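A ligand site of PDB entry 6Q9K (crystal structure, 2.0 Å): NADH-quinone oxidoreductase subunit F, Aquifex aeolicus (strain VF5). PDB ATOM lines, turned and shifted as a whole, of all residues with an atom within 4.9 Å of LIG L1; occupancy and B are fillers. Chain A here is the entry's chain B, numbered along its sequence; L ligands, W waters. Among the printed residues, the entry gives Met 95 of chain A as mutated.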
ATOM      1  N   GLY A  66     -19.618  -5.143  25.536  1.00  0.00           N
ATOM      2  CA  GLY A  66     -19.615  -6.531  25.056  1.00  0.00           C
ATOM      3  C   GLY A  66     -19.376  -7.503  26.201  1.00  0.00           C
ATOM      4  O   GLY A  66     -19.820  -8.661  26.092  1.00  0.00           O
ATOM      5  N   GLY A  67     -18.675  -7.072  27.255  1.00  0.00           N
ATOM      6  CA  GLY A  67     -18.500  -7.879  28.479  1.00  0.00           C
ATOM      7  C   GLY A  67     -17.112  -7.780  29.086  1.00  0.00           C
ATOM      8  O   GLY A  67     -17.005  -8.018  30.309  1.00  0.00           O
ATOM      9  N   ALA A  68     -16.073  -7.475  28.287  1.00  0.00           N
ATOM     10  CA  ALA A  68     -14.677  -7.381  28.773  1.00  0.00           C
ATOM     11  C   ALA A  68     -14.420  -6.008  29.395  1.00  0.00           C
ATOM     12  O   ALA A  68     -13.468  -5.909  30.190  1.00  0.00           O
ATOM     13  CB  ALA A  68     -13.686  -7.656  27.674  1.00  0.00           C
ATOM     14  N   PHE A  70     -13.157  -3.223  28.058  1.00  0.00           N
ATOM     15  CA  PHE A  70     -11.931  -2.523  27.591  1.00  0.00           C
ATOM     16  C   PHE A  70     -12.271  -1.058  27.273  1.00  0.00           C
ATOM     17  O   PHE A  70     -13.289  -0.779  26.654  1.00  0.00           O
ATOM     18  CB  PHE A  70     -11.322  -3.223  26.370  1.00  0.00           C
ATOM     19  CG  PHE A  70      -9.957  -2.721  26.013  1.00  0.00           C
ATOM     20  CD1 PHE A  70      -8.828  -3.280  26.574  1.00  0.00           C
ATOM     21  CD2 PHE A  70      -9.800  -1.658  25.132  1.00  0.00           C
ATOM     22  CE1 PHE A  70      -7.558  -2.803  26.255  1.00  0.00           C
ATOM     23  CE2 PHE A  70      -8.530  -1.193  24.807  1.00  0.00           C
ATOM     24  CZ  PHE A  70      -7.412  -1.762  25.368  1.00  0.00           C
ATOM     25  N   LYS A  75      -9.038   1.842  22.758  1.00  0.00           N
ATOM     26  CA  LYS A  75      -9.062   0.887  21.618  1.00  0.00           C
ATOM     27  C   LYS A  75      -8.933   1.680  20.308  1.00  0.00           C
ATOM     28  O   LYS A  75      -8.092   1.309  19.482  1.00  0.00           O
ATOM     29  CB  LYS A  75     -10.333   0.032  21.599  1.00  0.00           C
ATOM     30  CG  LYS A  75     -10.280  -1.131  20.615  1.00  0.00           C
ATOM     31  CD  LYS A  75     -11.570  -1.897  20.483  1.00  0.00           C
ATOM     32  CE  LYS A  75     -12.031  -2.555  21.765  1.00  0.00           C
ATOM     33  NZ  LYS A  75     -13.264  -3.352  21.547  1.00  0.00           N
ATOM     34  N   PHE A  78      -5.409   3.001  19.516  1.00  0.00           N
ATOM     35  CA  PHE A  78      -4.491   1.936  19.038  1.00  0.00           C
ATOM     36  C   PHE A  78      -4.701   1.743  17.538  1.00  0.00           C
ATOM     37  O   PHE A  78      -3.697   1.637  16.798  1.00  0.00           O
ATOM     38  CB  PHE A  78      -4.702   0.592  19.766  1.00  0.00           C
ATOM     39  CG  PHE A  78      -3.977   0.417  21.071  1.00  0.00           C
ATOM     40  CD1 PHE A  78      -2.580   0.367  21.113  1.00  0.00           C
ATOM     41  CD2 PHE A  78      -4.671   0.250  22.264  1.00  0.00           C
ATOM     42  CE1 PHE A  78      -1.915   0.184  22.313  1.00  0.00           C
ATOM     43  CE2 PHE A  78      -4.001   0.071  23.458  1.00  0.00           C
ATOM     44  CZ  PHE A  78      -2.628   0.040  23.493  1.00  0.00           C
ATOM     45  N   GLU A  94     -24.420 -11.297  19.981  1.00  0.00           N
ATOM     46  CA  GLU A  94     -25.108 -11.549  21.281  1.00  0.00           C
ATOM     47  C   GLU A  94     -25.637 -12.980  21.402  1.00  0.00           C
ATOM     48  O   GLU A  94     -26.819 -13.227  21.081  1.00  0.00           O
ATOM     49  CB  GLU A  94     -26.257 -10.546  21.439  1.00  0.00           C
ATOM     50  CG  GLU A  94     -26.995 -10.723  22.747  1.00  0.00           C
ATOM     51  CD  GLU A  94     -27.893  -9.551  23.082  1.00  0.00           C
ATOM     52  OE1 GLU A  94     -28.924  -9.396  22.407  1.00  0.00           O
ATOM     53  OE2 GLU A  94     -27.514  -8.772  23.980  1.00  0.00           O
ATOM     54  N   MET A  95     -24.815 -13.919  21.896  1.00  0.00           N
ATOM     55  CA  MET A  95     -25.228 -15.336  22.042  1.00  0.00           C
ATOM     56  C   MET A  95     -24.864 -15.897  23.429  1.00  0.00           C
ATOM     57  O   MET A  95     -25.014 -17.109  23.603  1.00  0.00           O
ATOM     58  CB  MET A  95     -24.606 -16.218  20.956  1.00  0.00           C
ATOM     59  CG  MET A  95     -25.363 -16.118  19.652  1.00  0.00           C
ATOM     60  SD  MET A  95     -24.652 -17.067  18.317  1.00  0.00           S
ATOM     61  CE  MET A  95     -25.102 -18.734  18.798  1.00  0.00           C
ATOM     62  N   GLU A  96     -24.441 -15.046  24.375  1.00  0.00           N
ATOM     63  CA  GLU A  96     -24.233 -15.450  25.794  1.00  0.00           C
ATOM     64  C   GLU A  96     -25.581 -15.828  26.390  1.00  0.00           C
ATOM     65  O   GLU A  96     -26.546 -15.082  26.255  1.00  0.00           O
ATOM     66  CB  GLU A  96     -23.608 -14.312  26.606  1.00  0.00           C
ATOM     67  CG  GLU A  96     -23.147 -14.721  27.990  1.00  0.00           C
ATOM     68  CD  GLU A  96     -21.864 -15.533  28.018  1.00  0.00           C
ATOM     69  OE1 GLU A  96     -21.445 -16.028  26.956  1.00  0.00           O
ATOM     70  OE2 GLU A  96     -21.279 -15.675  29.114  1.00  0.00           O
ATOM     71  N   THR A  99     -28.476 -13.313  27.837  1.00  0.00           N
ATOM     72  CA  THR A  99     -28.069 -11.984  27.288  1.00  0.00           C
ATOM     73  C   THR A  99     -28.974 -11.609  26.107  1.00  0.00           C
ATOM     74  O   THR A  99     -28.934 -12.286  25.056  1.00  0.00           O
ATOM     75  CB  THR A  99     -26.563 -11.957  26.987  1.00  0.00           C
ATOM     76  OG1 THR A  99     -25.899 -12.533  28.105  1.00  0.00           O
ATOM     77  CG2 THR A  99     -26.060 -10.556  26.732  1.00  0.00           C
ATOM     78  N   ASP A 102     -28.661  -6.287  23.641  1.00  0.00           N
ATOM     79  CA  ASP A 102     -28.311  -5.614  22.355  1.00  0.00           C
ATOM     80  C   ASP A 102     -29.510  -5.624  21.403  1.00  0.00           C
ATOM     81  O   ASP A 102     -29.700  -4.619  20.659  1.00  0.00           O
ATOM     82  CB  ASP A 102     -27.111  -6.290  21.670  1.00  0.00           C
ATOM     83  CG  ASP A 102     -25.821  -6.232  22.471  1.00  0.00           C
ATOM     84  OD1 ASP A 102     -25.745  -5.386  23.404  1.00  0.00           O
ATOM     85  OD2 ASP A 102     -24.900  -7.018  22.175  1.00  0.00           O
ATOM     86  N   TYR A 179     -21.767 -19.484  18.454  1.00  0.00           N
ATOM     87  CA  TYR A 179     -21.433 -18.604  19.600  1.00  0.00           C
ATOM     88  C   TYR A 179     -20.039 -17.994  19.398  1.00  0.00           C
ATOM     89  O   TYR A 179     -19.841 -16.801  19.690  1.00  0.00           O
ATOM     90  CB  TYR A 179     -21.485 -19.439  20.887  1.00  0.00           C
ATOM     91  CG  TYR A 179     -20.909 -18.841  22.142  1.00  0.00           C
ATOM     92  CD1 TYR A 179     -21.543 -17.810  22.810  1.00  0.00           C
ATOM     93  CD2 TYR A 179     -19.791 -19.397  22.738  1.00  0.00           C
ATOM     94  CE1 TYR A 179     -21.049 -17.327  24.004  1.00  0.00           C
ATOM     95  CE2 TYR A 179     -19.285 -18.929  23.932  1.00  0.00           C
ATOM     96  CZ  TYR A 179     -19.921 -17.874  24.572  1.00  0.00           C
ATOM     97  OH  TYR A 179     -19.437 -17.424  25.766  1.00  0.00           O
ATOM     98  N   GLU A 184     -14.173 -11.638  18.514  1.00  0.00           N
ATOM     99  CA  GLU A 184     -13.909 -10.592  17.497  1.00  0.00           C
ATOM    100  C   GLU A 184     -13.080 -11.146  16.333  1.00  0.00           C
ATOM    101  O   GLU A 184     -13.349 -10.743  15.198  1.00  0.00           O
ATOM    102  CB  GLU A 184     -13.217  -9.386  18.137  1.00  0.00           C
ATOM    103  CG  GLU A 184     -11.944  -9.709  18.891  1.00  0.00           C
ATOM    104  CD  GLU A 184     -11.249  -8.475  19.438  1.00  0.00           C
ATOM    105  OE1 GLU A 184     -11.838  -7.372  19.313  1.00  0.00           O
ATOM    106  OE2 GLU A 184     -10.141  -8.619  19.983  1.00  0.00           O
ATOM    107  N   TYR A 204      -3.950  -7.861  17.993  1.00  0.00           N
ATOM    108  CA  TYR A 204      -5.368  -7.487  18.183  1.00  0.00           C
ATOM    109  C   TYR A 204      -5.877  -6.889  16.877  1.00  0.00           C
ATOM    110  O   TYR A 204      -5.090  -6.401  16.055  1.00  0.00           O
ATOM    111  CB  TYR A 204      -5.521  -6.557  19.384  1.00  0.00           C
ATOM    112  CG  TYR A 204      -5.217  -7.227  20.703  1.00  0.00           C
ATOM    113  CD1 TYR A 204      -6.174  -7.986  21.362  1.00  0.00           C
ATOM    114  CD2 TYR A 204      -3.951  -7.159  21.257  1.00  0.00           C
ATOM    115  CE1 TYR A 204      -5.892  -8.633  22.554  1.00  0.00           C
ATOM    116  CE2 TYR A 204      -3.645  -7.801  22.441  1.00  0.00           C
ATOM    117  CZ  TYR A 204      -4.621  -8.548  23.093  1.00  0.00           C
ATOM    118  OH  TYR A 204      -4.317  -9.178  24.256  1.00  0.00           O
ATOM    119  N   PRO A 205      -7.206  -6.922  16.643  1.00  0.00           N
ATOM    120  CA  PRO A 205      -7.777  -6.424  15.396  1.00  0.00           C
ATOM    121  C   PRO A 205      -7.348  -4.991  15.037  1.00  0.00           C
ATOM    122  O   PRO A 205      -7.225  -4.712  13.858  1.00  0.00           O
ATOM    123  CB  PRO A 205      -9.293  -6.497  15.676  1.00  0.00           C
ATOM    124  CG  PRO A 205      -9.427  -7.619  16.663  1.00  0.00           C
ATOM    125  CD  PRO A 205      -8.226  -7.441  17.564  1.00  0.00           C
ATOM    126  N   VAL A 206      -7.149  -4.126  16.045  1.00  0.00           N
ATOM    127  CA  VAL A 206      -6.761  -2.702  15.843  1.00  0.00           C
ATOM    128  C   VAL A 206      -5.408  -2.623  15.128  1.00  0.00           C
ATOM    129  O   VAL A 206      -5.134  -1.587  14.485  1.00  0.00           O
ATOM    130  CB  VAL A 206      -6.748  -1.898  17.160  1.00  0.00           C
ATOM    131  CG1 VAL A 206      -8.151  -1.760  17.734  1.00  0.00           C
ATOM    132  CG2 VAL A 206      -5.785  -2.492  18.186  1.00  0.00           C
ATOM    133  N   VAL A 217     -13.443  -3.572  16.545  1.00  0.00           N
ATOM    134  CA  VAL A 217     -14.681  -4.330  16.858  1.00  0.00           C
ATOM    135  C   VAL A 217     -15.249  -3.738  18.142  1.00  0.00           C
ATOM    136  O   VAL A 217     -14.508  -3.694  19.134  1.00  0.00           O
ATOM    137  CB  VAL A 217     -14.436  -5.842  16.994  1.00  0.00           C
ATOM    138  CG1 VAL A 217     -15.752  -6.583  17.274  1.00  0.00           C
ATOM    139  CG2 VAL A 217     -13.747  -6.415  15.756  1.00  0.00           C
ATOM    140  N   ASN A 219     -19.111  -3.633  20.527  1.00  0.00           N
ATOM    141  CA  ASN A 219     -20.447  -4.175  20.855  1.00  0.00           C
ATOM    142  C   ASN A 219     -21.507  -3.121  20.529  1.00  0.00           C
ATOM    143  O   ASN A 219     -21.215  -1.916  20.677  1.00  0.00           O
ATOM    144  CB  ASN A 219     -20.452  -4.581  22.335  1.00  0.00           C
ATOM    145  CG  ASN A 219     -21.819  -4.973  22.854  1.00  0.00           C
ATOM    146  OD1 ASN A 219     -22.451  -4.195  23.566  1.00  0.00           O
ATOM    147  ND2 ASN A 219     -22.250  -6.168  22.498  1.00  0.00           N
ATOM    148  N   LEU A 296     -20.391 -16.998  32.494  1.00  0.00           N
ATOM    149  CA  LEU A 296     -19.034 -16.513  32.880  1.00  0.00           C
ATOM    150  C   LEU A 296     -18.779 -16.677  34.381  1.00  0.00           C
ATOM    151  O   LEU A 296     -17.713 -17.233  34.732  1.00  0.00           O
ATOM    152  CB  LEU A 296     -18.914 -15.042  32.480  1.00  0.00           C
ATOM    153  CG  LEU A 296     -17.551 -14.398  32.716  1.00  0.00           C
ATOM    154  CD1 LEU A 296     -16.470 -15.077  31.886  1.00  0.00           C
ATOM    155  CD2 LEU A 296     -17.603 -12.910  32.390  1.00  0.00           C
ATOM    156  N   GLY A 317     -18.766  -8.298  33.419  1.00  0.00           N
ATOM    157  CA  GLY A 317     -19.327  -9.115  32.321  1.00  0.00           C
ATOM    158  C   GLY A 317     -20.279  -8.311  31.471  1.00  0.00           C
ATOM    159  O   GLY A 317     -20.041  -7.119  31.295  1.00  0.00           O
ATOM    160  N   THR A 318     -21.331  -8.949  30.957  1.00  0.00           N
ATOM    161  CA  THR A 318     -22.350  -8.349  30.061  1.00  0.00           C
ATOM    162  C   THR A 318     -23.346  -7.515  30.881  1.00  0.00           C
ATOM    163  O   THR A 318     -24.093  -6.745  30.273  1.00  0.00           O
ATOM    164  CB  THR A 318     -23.065  -9.430  29.244  1.00  0.00           C
ATOM    165  OG1 THR A 318     -23.608 -10.364  30.176  1.00  0.00           O
ATOM    166  CG2 THR A 318     -22.193 -10.169  28.264  1.00  0.00           C
ATOM    167  N   GLY A 393     -11.061 -16.580  24.610  1.00  0.00           N
ATOM    168  CA  GLY A 393     -11.730 -16.500  25.914  1.00  0.00           C
ATOM    169  C   GLY A 393     -12.623 -17.699  26.220  1.00  0.00           C
ATOM    170  O   GLY A 393     -12.901 -17.895  27.403  1.00  0.00           O
HETATM  171  P1  LIG L   1     -10.417  -9.189  26.013  1.00  0.00           P
HETATM  172  O1  LIG L   1     -10.392  -8.617  27.382  1.00  0.00           O
HETATM  173  O2  LIG L   1      -9.253 -10.037  25.627  1.00  0.00           O
HETATM  174  O3  LIG L   1     -10.498  -8.004  24.891  1.00  0.00           O
HETATM  175  C1  LIG L   1     -11.522  -6.991  24.982  1.00  0.00           C
HETATM  176  C2  LIG L   1     -11.374  -6.021  23.848  1.00  0.00           C
HETATM  177  O4  LIG L   1     -10.211  -5.190  24.103  1.00  0.00           O
HETATM  178  C3  LIG L   1     -11.173  -6.630  22.460  1.00  0.00           C
HETATM  179  O5  LIG L   1     -11.803  -5.865  21.439  1.00  0.00           O
HETATM  180  C4  LIG L   1      -9.651  -6.618  22.300  1.00  0.00           C
HETATM  181  O6  LIG L   1      -9.263  -6.536  20.938  1.00  0.00           O
HETATM  182  C5  LIG L   1      -9.272  -5.329  23.047  1.00  0.00           C
HETATM  183  N1  LIG L   1      -7.931  -5.368  23.620  1.00  0.00           N
HETATM  184  C6  LIG L   1      -7.509  -6.069  24.717  1.00  0.00           C
HETATM  185  N2  LIG L   1      -6.230  -5.949  24.980  1.00  0.00           N
HETATM  186  C7  LIG L   1      -5.765  -5.113  23.973  1.00  0.00           C
HETATM  187  C8  LIG L   1      -4.491  -4.607  23.661  1.00  0.00           C
HETATM  188  N3  LIG L   1      -3.382  -4.918  24.355  1.00  0.00           N
HETATM  189  N4  LIG L   1      -4.380  -3.793  22.585  1.00  0.00           N
HETATM  190  C9  LIG L   1      -5.476  -3.511  21.883  1.00  0.00           C
HETATM  191  N5  LIG L   1      -6.735  -3.927  22.067  1.00  0.00           N
HETATM  192  C10 LIG L   1      -6.806  -4.735  23.135  1.00  0.00           C
HETATM  193  O7  LIG L   1     -11.726 -10.071  25.840  1.00  0.00           O
HETATM  194  P2  LIG L   1     -12.454 -10.929  24.719  1.00  0.00           P
HETATM  195  O8  LIG L   1     -11.882 -12.323  24.769  1.00  0.00           O
HETATM  196  O9  LIG L   1     -12.516 -10.247  23.393  1.00  0.00           O
HETATM  197  O10 LIG L   1     -13.925 -10.998  25.380  1.00  0.00           O
HETATM  198  C11 LIG L   1     -14.292 -11.721  26.582  1.00  0.00           C
HETATM  199  C12 LIG L   1     -15.679 -11.288  26.983  1.00  0.00           C
HETATM  200  O11 LIG L   1     -16.634 -11.679  25.985  1.00  0.00           O
HETATM  201  C13 LIG L   1     -16.199 -11.904  28.288  1.00  0.00           C
HETATM  202  O12 LIG L   1     -15.923 -11.031  29.372  1.00  0.00           O
HETATM  203  C14 LIG L   1     -17.712 -12.069  28.045  1.00  0.00           C
HETATM  204  O13 LIG L   1     -18.450 -11.263  28.958  1.00  0.00           O
HETATM  205  C15 LIG L   1     -17.902 -11.562  26.604  1.00  0.00           C
HETATM  206  N6  LIG L   1     -18.887 -12.296  25.821  1.00  0.00           N
HETATM  207  C16 LIG L   1     -20.101 -11.678  25.410  1.00  0.00           C
HETATM  208  C17 LIG L   1     -21.048 -12.333  24.703  1.00  0.00           C
HETATM  209  C18 LIG L   1     -22.300 -11.619  24.377  1.00  0.00           C
HETATM  210  O14 LIG L   1     -23.285 -12.257  23.982  1.00  0.00           O
HETATM  211  N7  LIG L   1     -22.337 -10.291  24.519  1.00  0.00           N
HETATM  212  C19 LIG L   1     -20.862 -13.756  24.324  1.00  0.00           C
HETATM  213  C20 LIG L   1     -19.546 -14.295  24.774  1.00  0.00           C
HETATM  214  C21 LIG L   1     -18.671 -13.595  25.469  1.00  0.00           C
HETATM  215  N1  LG2 L   2     -18.712  -9.414  22.184  1.00  0.00           N
HETATM  216  C1  LG2 L   2     -19.898  -8.939  21.696  1.00  0.00           C
HETATM  217  O1  LG2 L   2     -20.094  -7.719  21.560  1.00  0.00           O
HETATM  218  N2  LG2 L   2     -20.888  -9.847  21.303  1.00  0.00           N
HETATM  219  C2  LG2 L   2     -20.781 -11.224  21.308  1.00  0.00           C
HETATM  220  O2  LG2 L   2     -21.722 -11.917  20.940  1.00  0.00           O
HETATM  221  C3  LG2 L   2     -19.483 -11.714  21.801  1.00  0.00           C
HETATM  222  N3  LG2 L   2     -19.265 -13.003  21.788  1.00  0.00           N
HETATM  223  C4  LG2 L   2     -18.028 -13.464  22.240  1.00  0.00           C
HETATM  224  C5  LG2 L   2     -17.787 -14.838  22.263  1.00  0.00           C
HETATM  225  C6  LG2 L   2     -16.598 -15.350  22.773  1.00  0.00           C
HETATM  226  C7  LG2 L   2     -16.380 -16.843  22.804  1.00  0.00           C
HETATM  227  C8  LG2 L   2     -15.617 -14.462  23.258  1.00  0.00           C
HETATM  228  C9  LG2 L   2     -14.344 -14.973  23.886  1.00  0.00           C
HETATM  229  C10 LG2 L   2     -15.835 -13.095  23.192  1.00  0.00           C
HETATM  230  C11 LG2 L   2     -17.035 -12.580  22.704  1.00  0.00           C
HETATM  231  N4  LG2 L   2     -17.312 -11.183  22.668  1.00  0.00           N
HETATM  232  C12 LG2 L   2     -18.526 -10.730  22.216  1.00  0.00           C
HETATM  233  C13 LG2 L   2     -16.288 -10.184  23.003  1.00  0.00           C
HETATM  234  C14 LG2 L   2     -15.552  -9.692  21.757  1.00  0.00           C
HETATM  235  O3  LG2 L   2     -14.489 -10.582  21.424  1.00  0.00           O
HETATM  236  C15 LG2 L   2     -15.003  -8.274  21.975  1.00  0.00           C
HETATM  237  O4  LG2 L   2     -14.343  -8.208  23.224  1.00  0.00           O
HETATM  238  C16 LG2 L   2     -16.052  -7.165  21.925  1.00  0.00           C
HETATM  239  O5  LG2 L   2     -16.962  -7.365  20.839  1.00  0.00           O
HETATM  240  C17 LG2 L   2     -15.393  -5.809  21.815  1.00  0.00           C
HETATM  241  O6  LG2 L   2     -16.404  -4.799  21.941  1.00  0.00           O
HETATM  242  P1  LG2 L   2     -16.522  -3.920  23.262  1.00  0.00           P
HETATM  243  O7  LG2 L   2     -17.130  -4.741  24.365  1.00  0.00           O
HETATM  244  O8  LG2 L   2     -15.096  -3.432  23.618  1.00  0.00           O
HETATM  245  O9  LG2 L   2     -17.333  -2.694  22.837  1.00  0.00           O
HETATM  246  O   HOH W   1      -8.647  -4.473  19.587  1.00  0.00           O
HETATM  247  O   HOH W   2      -2.949  -6.919  26.358  1.00  0.00           O
HETATM  248  O   HOH W   3     -10.919 -13.292  27.062  1.00  0.00           O
HETATM  249  O   HOH W   4     -16.940 -15.811  27.396  1.00  0.00           O
HETATM  250  O   HOH W   5     -20.384 -13.233  29.840  1.00  0.00           O
HETATM  251  O   HOH W   6     -24.673  -8.599  24.372  1.00  0.00           O
HETATM  252  O   HOH W   7      -5.433  -7.085  27.272  1.00  0.00           O
HETATM  253  O   HOH W   8     -13.522 -11.580  30.388  1.00  0.00           O
HETATM  254  O   HOH W   9     -10.351 -10.840  21.735  1.00  0.00           O
HETATM  255  O   HOH W  10     -10.942 -14.064  22.979  1.00  0.00           O
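Water W10 bridges O8 of LIG L1 and N of Gly 393. Water W9 lies within hydrogen-bond range of O9 of LIG L1 (2.8 Å) and OE2 of Glu 184 (2.8 Å). Water W2 bridges N3 of LIG L1 and OH of Tyr 204. Water W6 lies within hydrogen-bond range of OD2 of Asp 102 (2.7 Å), OE2 of Glu 94 (2.9 Å) and N7 of LIG L1 (2.9 Å). Water W5 lies within hydrogen-bond range of OE2 of Glu 96 (2.7 Å) and O13 of LIG L1 (2.9 Å).
An oxygen (O6) of LIG L1 sits at hydrogen-bond distance from the side-chain carboxylate (OE2) of Glu 184 (2.5 Å). The side-chain amino group of Lys 75 lies within hydrogen-bond range of an oxygen (O5) of LIG L1, 2.9 Å away. An oxygen (O14) of LIG L1 is in hydrogen-bond range of the backbone NH (N) of Glu 96 (3.0 Å). The backbone NH of Met 95 lies within hydrogen-bond range of an oxygen (O14) of LIG L1. O of Gly 66 lies close to N7 of LIG L1, at 3.4 Å. An oxygen (O12) of LIG L1 lies within hydrogen-bond range of the backbone carbonyl oxygen of Gly 67 (3.3 Å). The backbone NH (N) of Glu 184 lies within hydrogen-bond range of an oxygen (O3) of LG2 L2, at 3.1 Å. O8 of LG2 L2 lies within salt-bridge range of NZ of Lys 75 (2.8 Å). O7 of LG2 L2 is in hydrogen-bond range of N of Gly 66. N of Glu 94 lies within hydrogen-bond range of O2 of LG2 L2 (2.9 Å). N of Asn 219 sits at hydrogen-bond distance from O9 of LG2 L2 (3.1 Å). The side-chain amide nitrogen (ND2) of Asn 219 lies within hydrogen-bond range of an oxygen (O1) of LG2 L2 (2.8 Å).
Ala 68 touches LIG L1 (CB to O1, 3.4 Å). CG of Phe 70 touches O4 of LIG L1, at 3.1 Å. Phe 78 touches LIG L1. Glu 94 touches LIG L1 (CA to O14, 3.3 Å). Tyr 179 touches LIG L1 (OH to C20, 3.3 Å). CD1 of Tyr 204 touches O6 of LIG L1 (3.4 Å). Pro 205 touches LIG L1 (CD to O6, 3.6 Å). Val 206 touches LIG L1. CD2 of Leu 296 touches O13 of LIG L1, at 3.9 Å. Thr 318 touches LIG L1. Hydrophobic or aromatic side chains that line LIG L1: Ala 68, Phe 70, Phe 78, Tyr 179, Tyr 204, Pro 205, Val 206 and Leu 296. Within 4 Å of LIG L1: Gly 66, Gly 67, Ala 68, Phe 70, Lys 75, Phe 78, Glu 94, Met 95, Glu 96, Tyr 179, Glu 184, Tyr 204, Pro 205, Val 206, Leu 296 and Thr 318.
NZ of Lys 75 is in hydrogen-bond range of O of Val 217 (2.7 Å). OE1 of Glu 96 lies within hydrogen-bond range of OH of Tyr 179 (2.7 Å). The side-chain hydroxyl (OG1) of Thr 99 sits close to the backbone carbonyl oxygen (O) of Glu 96, at 3.2 Å. N of Tyr 179 lies close to SD of Met 95, at 3.8 Å. The side-chain carboxylate (OE2) of Glu 94 sits at hydrogen-bond distance from the backbone NH (N) of Asp 102 (2.8 Å).
O9 of LIG L1 lies within hydrogen-bond range of O4 of LG2 L2, 2.7 Å away.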
